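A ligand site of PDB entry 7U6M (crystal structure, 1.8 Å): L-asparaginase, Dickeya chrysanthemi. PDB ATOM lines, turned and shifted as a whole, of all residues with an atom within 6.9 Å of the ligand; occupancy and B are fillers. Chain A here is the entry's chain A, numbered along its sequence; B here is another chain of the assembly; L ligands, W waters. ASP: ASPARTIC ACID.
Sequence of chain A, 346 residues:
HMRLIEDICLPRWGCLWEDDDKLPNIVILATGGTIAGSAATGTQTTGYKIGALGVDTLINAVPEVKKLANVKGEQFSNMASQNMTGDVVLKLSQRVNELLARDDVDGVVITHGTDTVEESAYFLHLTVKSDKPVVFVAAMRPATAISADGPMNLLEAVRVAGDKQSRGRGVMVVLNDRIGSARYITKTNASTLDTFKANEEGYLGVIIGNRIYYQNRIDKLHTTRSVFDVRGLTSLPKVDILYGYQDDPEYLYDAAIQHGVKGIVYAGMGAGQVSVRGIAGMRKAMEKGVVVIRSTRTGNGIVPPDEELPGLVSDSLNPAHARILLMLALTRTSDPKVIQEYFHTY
N of Ser 81 is in hydrogen-bond range of OXT of the ligand, 2.7 Å away.
The side-chain hydroxyl (OG) of Ser 81 sits at hydrogen-bond distance from an oxygen (O) of the ligand, 2.6 Å away.
N of Thr 114 lies within hydrogen-bond range of OD2 of the ligand, at 2.8 Å.
OG1 of Thr 114 lies within hydrogen-bond range of OD1 of the ligand (2.6 Å).
N of Asp 115 sits at hydrogen-bond distance from O of the ligand.
The side-chain carboxylate of Asp 115 is in salt-bridge range of a nitrogen (N) of the ligand.
N of Thr 34 sits at hydrogen-bond distance from OD2 of the ligand (3.1 Å).
The side-chain hydroxyl (OG1) of Thr 34 lies close to an oxygen (OD2) of the ligand (3.1 Å).
The side-chain amide oxygen of Gln 82 sits at hydrogen-bond distance from a nitrogen (N) of the ligand, at 2.9 Å.
O of Ala 139 sits close to OD1 of the ligand (3.1 Å).
OG of Ser 81 sits at hydrogen-bond distance from N of Asp 115 (3.2 Å).
OG1 of Thr 116 lies within hydrogen-bond range of O of Ser 81 (2.8 Å).
The side-chain hydroxyl of Thr 114 lies within hydrogen-bond range of the side-chain amino group of Lys 187, 2.7 Å away.
OE1 of Gln 82 sits close to OD2 of Asp 115 (3.5 Å).
OD1 of Asp 115 is in salt-bridge range of NZ of Lys 187 (2.8 Å).
OG1 of Thr 34 lies within hydrogen-bond range of OH of Tyr 48, at 2.5 Å.
The backbone carbonyl oxygen (O) of Met 79 sits at hydrogen-bond distance from the backbone NH (N) of Gly 33, 2.9 Å away.
SD of Met 140 is in hydrogen-bond range of NZ of Lys 187.
Residues that only touch the ligand: Gly 113 (3.2 Å), Ala 80 (3.3 Å), Gly 33 (3.3 Å), Ile 50 (3.9 Å) and Met 140 (3.96 Å).
11 residues have an atom within 4 Å of the ligand: Gly 33, Thr 34, Ile 50, Ala 80, Ser 81, Gln 82, Gly 113, Thr 114, Asp 115, Ala 139 and Met 140.
The nearest printed residue that does not touch the ligand is Gln 273 of chain B (4.1 Å).
Water W2 lies within hydrogen-bond range of OD1 of the ligand and O of Met 140.
Water W4 bridges N of the ligand (3.1 Å) and NE2 of Gln 273 of chain B (3.5 Å).
Water W1 lies within hydrogen-bond range of NE2 of Gln 82 (3.1 Å) and N of the ligand (3.2 Å).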
ATOM      1  N   GLY A  32      16.743  21.913   2.448  1.00  0.00           N
ATOM      2  CA  GLY A  32      16.877  23.107   3.305  1.00  0.00           C
ATOM      3  C   GLY A  32      18.173  23.078   4.135  1.00  0.00           C
ATOM      4  O   GLY A  32      19.246  22.833   3.553  1.00  0.00           O
ATOM      5  N   GLY A  33      18.051  23.454   5.398  1.00  0.00           N
ATOM      6  CA  GLY A  33      19.193  23.537   6.331  1.00  0.00           C
ATOM      7  C   GLY A  33      19.913  24.862   6.277  1.00  0.00           C
ATOM      8  O   GLY A  33      19.740  25.645   5.347  1.00  0.00           O
ATOM      9  N   THR A  34      20.854  25.049   7.218  1.00  0.00           N
ATOM     10  CA  THR A  34      21.735  26.229   7.291  1.00  0.00           C
ATOM     11  C   THR A  34      22.541  26.330   6.008  1.00  0.00           C
ATOM     12  O   THR A  34      22.928  27.480   5.667  1.00  0.00           O
ATOM     13  CB  THR A  34      22.587  26.165   8.562  1.00  0.00           C
ATOM     14  OG1 THR A  34      21.652  26.272   9.650  1.00  0.00           O
ATOM     15  CG2 THR A  34      23.627  27.261   8.623  1.00  0.00           C
ATOM     16  N   ILE A  35      22.873  25.219   5.344  1.00  0.00           N
ATOM     17  CA  ILE A  35      23.622  25.292   4.057  1.00  0.00           C
ATOM     18  C   ILE A  35      22.853  26.203   3.074  1.00  0.00           C
ATOM     19  O   ILE A  35      23.508  26.812   2.195  1.00  0.00           O
ATOM     20  CB  ILE A  35      23.842  23.899   3.463  1.00  0.00           C
ATOM     21  CG1 ILE A  35      24.805  23.896   2.271  1.00  0.00           C
ATOM     22  CG2 ILE A  35      22.539  23.170   3.146  1.00  0.00           C
ATOM     23  CD1 ILE A  35      25.358  22.513   1.964  1.00  0.00           C
ATOM     24  N   TYR A  48      19.069  34.277  10.887  1.00  0.00           N
ATOM     25  CA  TYR A  48      19.193  34.024   9.417  1.00  0.00           C
ATOM     26  C   TYR A  48      17.942  33.267   8.977  1.00  0.00           C
ATOM     27  O   TYR A  48      17.232  32.669   9.803  1.00  0.00           O
ATOM     28  CB  TYR A  48      20.466  33.338   8.909  1.00  0.00           C
ATOM     29  CG  TYR A  48      20.787  31.978   9.479  1.00  0.00           C
ATOM     30  CD1 TYR A  48      20.194  30.834   9.004  1.00  0.00           C
ATOM     31  CD2 TYR A  48      21.649  31.862  10.549  1.00  0.00           C
ATOM     32  CE1 TYR A  48      20.441  29.582   9.568  1.00  0.00           C
ATOM     33  CE2 TYR A  48      21.911  30.622  11.152  1.00  0.00           C
ATOM     34  CZ  TYR A  48      21.303  29.474  10.652  1.00  0.00           C
ATOM     35  OH  TYR A  48      21.538  28.257  11.243  1.00  0.00           O
ATOM     36  N   ILE A  50      16.071  30.315   6.756  1.00  0.00           N
ATOM     37  CA  ILE A  50      16.003  29.122   5.847  1.00  0.00           C
ATOM     38  C   ILE A  50      14.631  29.110   5.171  1.00  0.00           C
ATOM     39  O   ILE A  50      13.640  29.364   5.861  1.00  0.00           O
ATOM     40  CB  ILE A  50      16.279  27.814   6.607  1.00  0.00           C
ATOM     41  CG1 ILE A  50      17.644  27.858   7.331  1.00  0.00           C
ATOM     42  CG2 ILE A  50      16.155  26.623   5.663  1.00  0.00           C
ATOM     43  CD1 ILE A  50      17.851  26.755   8.353  1.00  0.00           C
ATOM     44  N   MET A  79      13.359  23.432   4.419  1.00  0.00           N
ATOM     45  CA  MET A  79      13.050  23.632   5.846  1.00  0.00           C
ATOM     46  C   MET A  79      14.327  23.497   6.702  1.00  0.00           C
ATOM     47  O   MET A  79      15.309  22.837   6.272  1.00  0.00           O
ATOM     48  CB  MET A  79      12.028  22.617   6.336  1.00  0.00           C
ATOM     49  CG  MET A  79      12.532  21.204   6.289  1.00  0.00           C
ATOM     50  SD  MET A  79      11.337  20.072   6.982  1.00  0.00           S
ATOM     51  CE  MET A  79      10.433  19.726   5.455  1.00  0.00           C
ATOM     52  N   ALA A  80      14.257  24.051   7.887  1.00  0.00           N
ATOM     53  CA  ALA A  80      15.255  23.815   8.971  1.00  0.00           C
ATOM     54  C   ALA A  80      15.009  22.376   9.446  1.00  0.00           C
ATOM     55  O   ALA A  80      13.814  22.004   9.671  1.00  0.00           O
ATOM     56  CB  ALA A  80      15.031  24.865  10.032  1.00  0.00           C
ATOM     57  N   SER A  81      16.071  21.575   9.595  1.00  0.00           N
ATOM     58  CA  SER A  81      15.929  20.121   9.834  1.00  0.00           C
ATOM     59  C   SER A  81      15.368  19.835  11.227  1.00  0.00           C
ATOM     60  O   SER A  81      14.928  18.705  11.431  1.00  0.00           O
ATOM     61  CB  SER A  81      17.237  19.388   9.583  1.00  0.00           C
ATOM     62  OG  SER A  81      18.130  19.555  10.701  1.00  0.00           O
ATOM     63  N   GLN A  82      15.314  20.794  12.141  1.00  0.00           N
ATOM     64  CA  GLN A  82      14.622  20.551  13.437  1.00  0.00           C
ATOM     65  C   GLN A  82      13.134  20.348  13.165  1.00  0.00           C
ATOM     66  O   GLN A  82      12.439  19.779  14.027  1.00  0.00           O
ATOM     67  CB  GLN A  82      14.812  21.665  14.470  1.00  0.00           C
ATOM     68  CG  GLN A  82      14.295  23.033  14.106  1.00  0.00           C
ATOM     69  CD  GLN A  82      15.274  23.886  13.336  1.00  0.00           C
ATOM     70  OE1 GLN A  82      16.129  23.391  12.602  1.00  0.00           O
ATOM     71  NE2 GLN A  82      15.188  25.196  13.540  1.00  0.00           N
ATOM     72  N   ASN A  83      12.662  20.767  11.980  1.00  0.00           N
ATOM     73  CA  ASN A  83      11.247  20.562  11.577  1.00  0.00           C
ATOM     74  C   ASN A  83      11.059  19.367  10.661  1.00  0.00           C
ATOM     75  O   ASN A  83       9.902  19.077  10.305  1.00  0.00           O
ATOM     76  CB  ASN A  83      10.690  21.861  11.033  1.00  0.00           C
ATOM     77  CG  ASN A  83      10.226  22.675  12.237  1.00  0.00           C
ATOM     78  OD1 ASN A  83       9.423  22.184  13.044  1.00  0.00           O
ATOM     79  ND2 ASN A  83      10.752  23.861  12.352  1.00  0.00           N
ATOM     80  N   HIS A 112      20.867  19.263   3.484  1.00  0.00           N
ATOM     81  CA  HIS A 112      20.008  19.031   4.668  1.00  0.00           C
ATOM     82  C   HIS A 112      20.558  19.847   5.827  1.00  0.00           C
ATOM     83  O   HIS A 112      21.767  20.155   5.816  1.00  0.00           O
ATOM     84  CB  HIS A 112      20.012  17.539   4.961  1.00  0.00           C
ATOM     85  CG  HIS A 112      18.923  17.042   5.863  1.00  0.00           C
ATOM     86  ND1 HIS A 112      18.981  17.190   7.247  1.00  0.00           N
ATOM     87  CD2 HIS A 112      17.891  16.206   5.606  1.00  0.00           C
ATOM     88  CE1 HIS A 112      17.972  16.528   7.785  1.00  0.00           C
ATOM     89  NE2 HIS A 112      17.263  15.911   6.792  1.00  0.00           N
ATOM     90  N   GLY A 113      19.713  20.154   6.771  1.00  0.00           N
ATOM     91  CA  GLY A 113      20.139  20.764   8.038  1.00  0.00           C
ATOM     92  C   GLY A 113      20.995  19.812   8.838  1.00  0.00           C
ATOM     93  O   GLY A 113      20.814  18.589   8.731  1.00  0.00           O
ATOM     94  N   THR A 114      21.932  20.349   9.625  1.00  0.00           N
ATOM     95  CA  THR A 114      22.813  19.505  10.445  1.00  0.00           C
ATOM     96  C   THR A 114      22.060  18.891  11.617  1.00  0.00           C
ATOM     97  O   THR A 114      22.466  17.815  12.050  1.00  0.00           O
ATOM     98  CB  THR A 114      24.007  20.310  10.984  1.00  0.00           C
ATOM     99  OG1 THR A 114      23.536  21.398  11.786  1.00  0.00           O
ATOM    100  CG2 THR A 114      24.910  20.811   9.875  1.00  0.00           C
ATOM    101  N   ASP A 115      21.012  19.556  12.124  1.00  0.00           N
ATOM    102  CA  ASP A 115      20.415  19.202  13.416  1.00  0.00           C
ATOM    103  C   ASP A 115      19.898  17.761  13.390  1.00  0.00           C
ATOM    104  O   ASP A 115      20.100  17.044  14.409  1.00  0.00           O
ATOM    105  CB  ASP A 115      19.362  20.190  13.824  1.00  0.00           C
ATOM    106  CG  ASP A 115      19.876  21.583  14.193  1.00  0.00           C
ATOM    107  OD1 ASP A 115      21.116  21.730  14.384  1.00  0.00           O
ATOM    108  OD2 ASP A 115      19.024  22.459  14.300  1.00  0.00           O
ATOM    109  N   THR A 116      19.247  17.316  12.315  1.00  0.00           N
ATOM    110  CA  THR A 116      18.656  15.957  12.270  1.00  0.00           C
ATOM    111  C   THR A 116      19.108  15.194  11.023  1.00  0.00           C
ATOM    112  O   THR A 116      18.521  14.123  10.706  1.00  0.00           O
ATOM    113  CB  THR A 116      17.125  15.979  12.381  1.00  0.00           C
ATOM    114  OG1 THR A 116      16.595  16.492  11.150  1.00  0.00           O
ATOM    115  CG2 THR A 116      16.648  16.777  13.555  1.00  0.00           C
ATOM    116  N   VAL A 117      20.209  15.602  10.390  1.00  0.00           N
ATOM    117  CA  VAL A 117      20.764  14.827   9.242  1.00  0.00           C
ATOM    118  C   VAL A 117      21.072  13.388   9.652  1.00  0.00           C
ATOM    119  O   VAL A 117      20.886  12.490   8.823  1.00  0.00           O
ATOM    120  CB  VAL A 117      21.976  15.525   8.586  1.00  0.00           C
ATOM    121  CG1 VAL A 117      23.227  15.472   9.469  1.00  0.00           C
ATOM    122  CG2 VAL A 117      22.248  14.960   7.216  1.00  0.00           C
ATOM    123  N   ALA A 138      25.730  19.157   4.475  1.00  0.00           N
ATOM    124  CA  ALA A 138      25.170  20.175   5.362  1.00  0.00           C
ATOM    125  C   ALA A 138      26.239  21.214   5.619  1.00  0.00           C
ATOM    126  O   ALA A 138      27.368  21.017   5.129  1.00  0.00           O
ATOM    127  CB  ALA A 138      24.610  19.523   6.634  1.00  0.00           C
ATOM    128  N   ALA A 139      25.888  22.265   6.342  1.00  0.00           N
ATOM    129  CA  ALA A 139      26.815  23.348   6.680  1.00  0.00           C
ATOM    130  C   ALA A 139      26.435  23.863   8.044  1.00  0.00           C
ATOM    131  O   ALA A 139      25.238  24.013   8.342  1.00  0.00           O
ATOM    132  CB  ALA A 139      26.813  24.453   5.657  1.00  0.00           C
ATOM    133  N   MET A 140      27.440  24.169   8.867  1.00  0.00           N
ATOM    134  CA  MET A 140      27.191  24.756  10.204  1.00  0.00           C
ATOM    135  C   MET A 140      27.048  26.267  10.125  1.00  0.00           C
ATOM    136  O   MET A 140      26.462  26.831  11.025  1.00  0.00           O
ATOM    137  CB  MET A 140      28.298  24.337  11.172  1.00  0.00           C
ATOM    138  CG  MET A 140      28.154  22.866  11.480  1.00  0.00           C
ATOM    139  SD  MET A 140      26.748  22.488  12.526  1.00  0.00           S
ATOM    140  CE  MET A 140      27.354  23.174  14.081  1.00  0.00           C
ATOM    141  N   ARG A 141      27.558  26.889   9.080  1.00  0.00           N
ATOM    142  CA  ARG A 141      27.452  28.358   8.904  1.00  0.00           C
ATOM    143  C   ARG A 141      26.557  28.622   7.693  1.00  0.00           C
ATOM    144  O   ARG A 141      26.592  27.878   6.726  1.00  0.00           O
ATOM    145  CB  ARG A 141      28.819  28.969   8.679  1.00  0.00           C
ATOM    146  CG  ARG A 141      29.757  28.890   9.881  1.00  0.00           C
ATOM    147  CD  ARG A 141      31.124  29.425   9.553  1.00  0.00           C
ATOM    148  NE  ARG A 141      32.013  29.324  10.720  1.00  0.00           N
ATOM    149  CZ  ARG A 141      33.339  29.351  10.667  1.00  0.00           C
ATOM    150  NH1 ARG A 141      33.987  29.469   9.520  1.00  0.00           N
ATOM    151  NH2 ARG A 141      34.036  29.226  11.781  1.00  0.00           N
ATOM    152  N   LYS A 187      26.033  14.331  15.159  1.00  0.00           N
ATOM    153  CA  LYS A 187      26.392  15.722  15.477  1.00  0.00           C
ATOM    154  C   LYS A 187      26.825  15.726  16.941  1.00  0.00           C
ATOM    155  O   LYS A 187      25.960  15.498  17.793  1.00  0.00           O
ATOM    156  CB  LYS A 187      25.204  16.647  15.193  1.00  0.00           C
ATOM    157  CG  LYS A 187      25.550  18.106  15.321  1.00  0.00           C
ATOM    158  CD  LYS A 187      24.408  19.055  14.950  1.00  0.00           C
ATOM    159  CE  LYS A 187      24.879  20.480  15.078  1.00  0.00           C
ATOM    160  NZ  LYS A 187      23.905  21.431  14.482  1.00  0.00           N
ATOM    161  N   ALA A 190      27.120  21.222  19.450  1.00  0.00           N
ATOM    162  CA  ALA A 190      26.010  22.133  19.108  1.00  0.00           C
ATOM    163  C   ALA A 190      26.407  23.026  17.933  1.00  0.00           C
ATOM    164  O   ALA A 190      25.512  23.344  17.114  1.00  0.00           O
ATOM    165  CB  ALA A 190      25.677  22.994  20.307  1.00  0.00           C
ATOM    166  N   MET B 269      17.870  19.388  19.536  1.00  0.00           N
ATOM    167  CA  MET B 269      18.512  19.096  18.247  1.00  0.00           C
ATOM    168  C   MET B 269      19.546  20.198  17.999  1.00  0.00           C
ATOM    169  O   MET B 269      19.223  21.388  18.124  1.00  0.00           O
ATOM    170  CB  MET B 269      17.440  19.073  17.135  1.00  0.00           C
ATOM    171  CG  MET B 269      16.441  17.963  17.380  1.00  0.00           C
ATOM    172  SD  MET B 269      14.990  18.003  16.259  1.00  0.00           S
ATOM    173  CE  MET B 269      13.898  19.052  17.227  1.00  0.00           C
ATOM    174  N   GLY B 270      20.776  19.813  17.700  1.00  0.00           N
ATOM    175  CA  GLY B 270      21.854  20.775  17.465  1.00  0.00           C
ATOM    176  C   GLY B 270      21.939  21.790  18.579  1.00  0.00           C
ATOM    177  O   GLY B 270      21.929  21.386  19.794  1.00  0.00           O
ATOM    178  N   ALA B 271      22.020  23.072  18.243  1.00  0.00           N
ATOM    179  CA  ALA B 271      22.189  24.160  19.218  1.00  0.00           C
ATOM    180  C   ALA B 271      20.843  24.529  19.870  1.00  0.00           C
ATOM    181  O   ALA B 271      20.383  25.662  19.695  1.00  0.00           O
ATOM    182  CB  ALA B 271      22.881  25.306  18.543  1.00  0.00           C
ATOM    183  N   GLN B 273      17.858  23.640  19.170  1.00  0.00           N
ATOM    184  CA  GLN B 273      16.827  23.986  18.170  1.00  0.00           C
ATOM    185  C   GLN B 273      15.577  23.161  18.441  1.00  0.00           C
ATOM    186  O   GLN B 273      15.639  22.013  18.947  1.00  0.00           O
ATOM    187  CB  GLN B 273      17.371  23.842  16.759  1.00  0.00           C
ATOM    188  CG  GLN B 273      18.587  24.709  16.517  1.00  0.00           C
ATOM    189  CD  GLN B 273      18.337  26.179  16.691  1.00  0.00           C
ATOM    190  OE1 GLN B 273      18.888  26.856  17.584  1.00  0.00           O
ATOM    191  NE2 GLN B 273      17.422  26.698  15.879  1.00  0.00           N
HETATM  192  N   ASP L   1      18.870  24.420  12.471  1.00  0.00           N
HETATM  193  CA  ASP L   1      19.696  24.159  11.237  1.00  0.00           C
HETATM  194  C   ASP L   1      19.125  22.928  10.533  1.00  0.00           C
HETATM  195  O   ASP L   1      19.379  21.775  11.022  1.00  0.00           O
HETATM  196  CB  ASP L   1      21.166  23.969  11.609  1.00  0.00           C
HETATM  197  CG  ASP L   1      22.170  23.635  10.515  1.00  0.00           C
HETATM  198  OD1 ASP L   1      23.394  23.812  10.808  1.00  0.00           O
HETATM  199  OD2 ASP L   1      21.794  23.143   9.407  1.00  0.00           O
HETATM  200  OXT ASP L   1      18.397  23.032   9.496  1.00  0.00           O
HETATM  201  O   HOH W   1      17.193  27.103  12.200  1.00  0.00           O
HETATM  202  O   HOH W   2      24.443  25.645  12.367  1.00  0.00           O
HETATM  203  O   HOH W   3      22.904  22.611   6.812  1.00  0.00           O
HETATM  204  O   HOH W   4      20.527  26.292  14.386  1.00  0.00           O
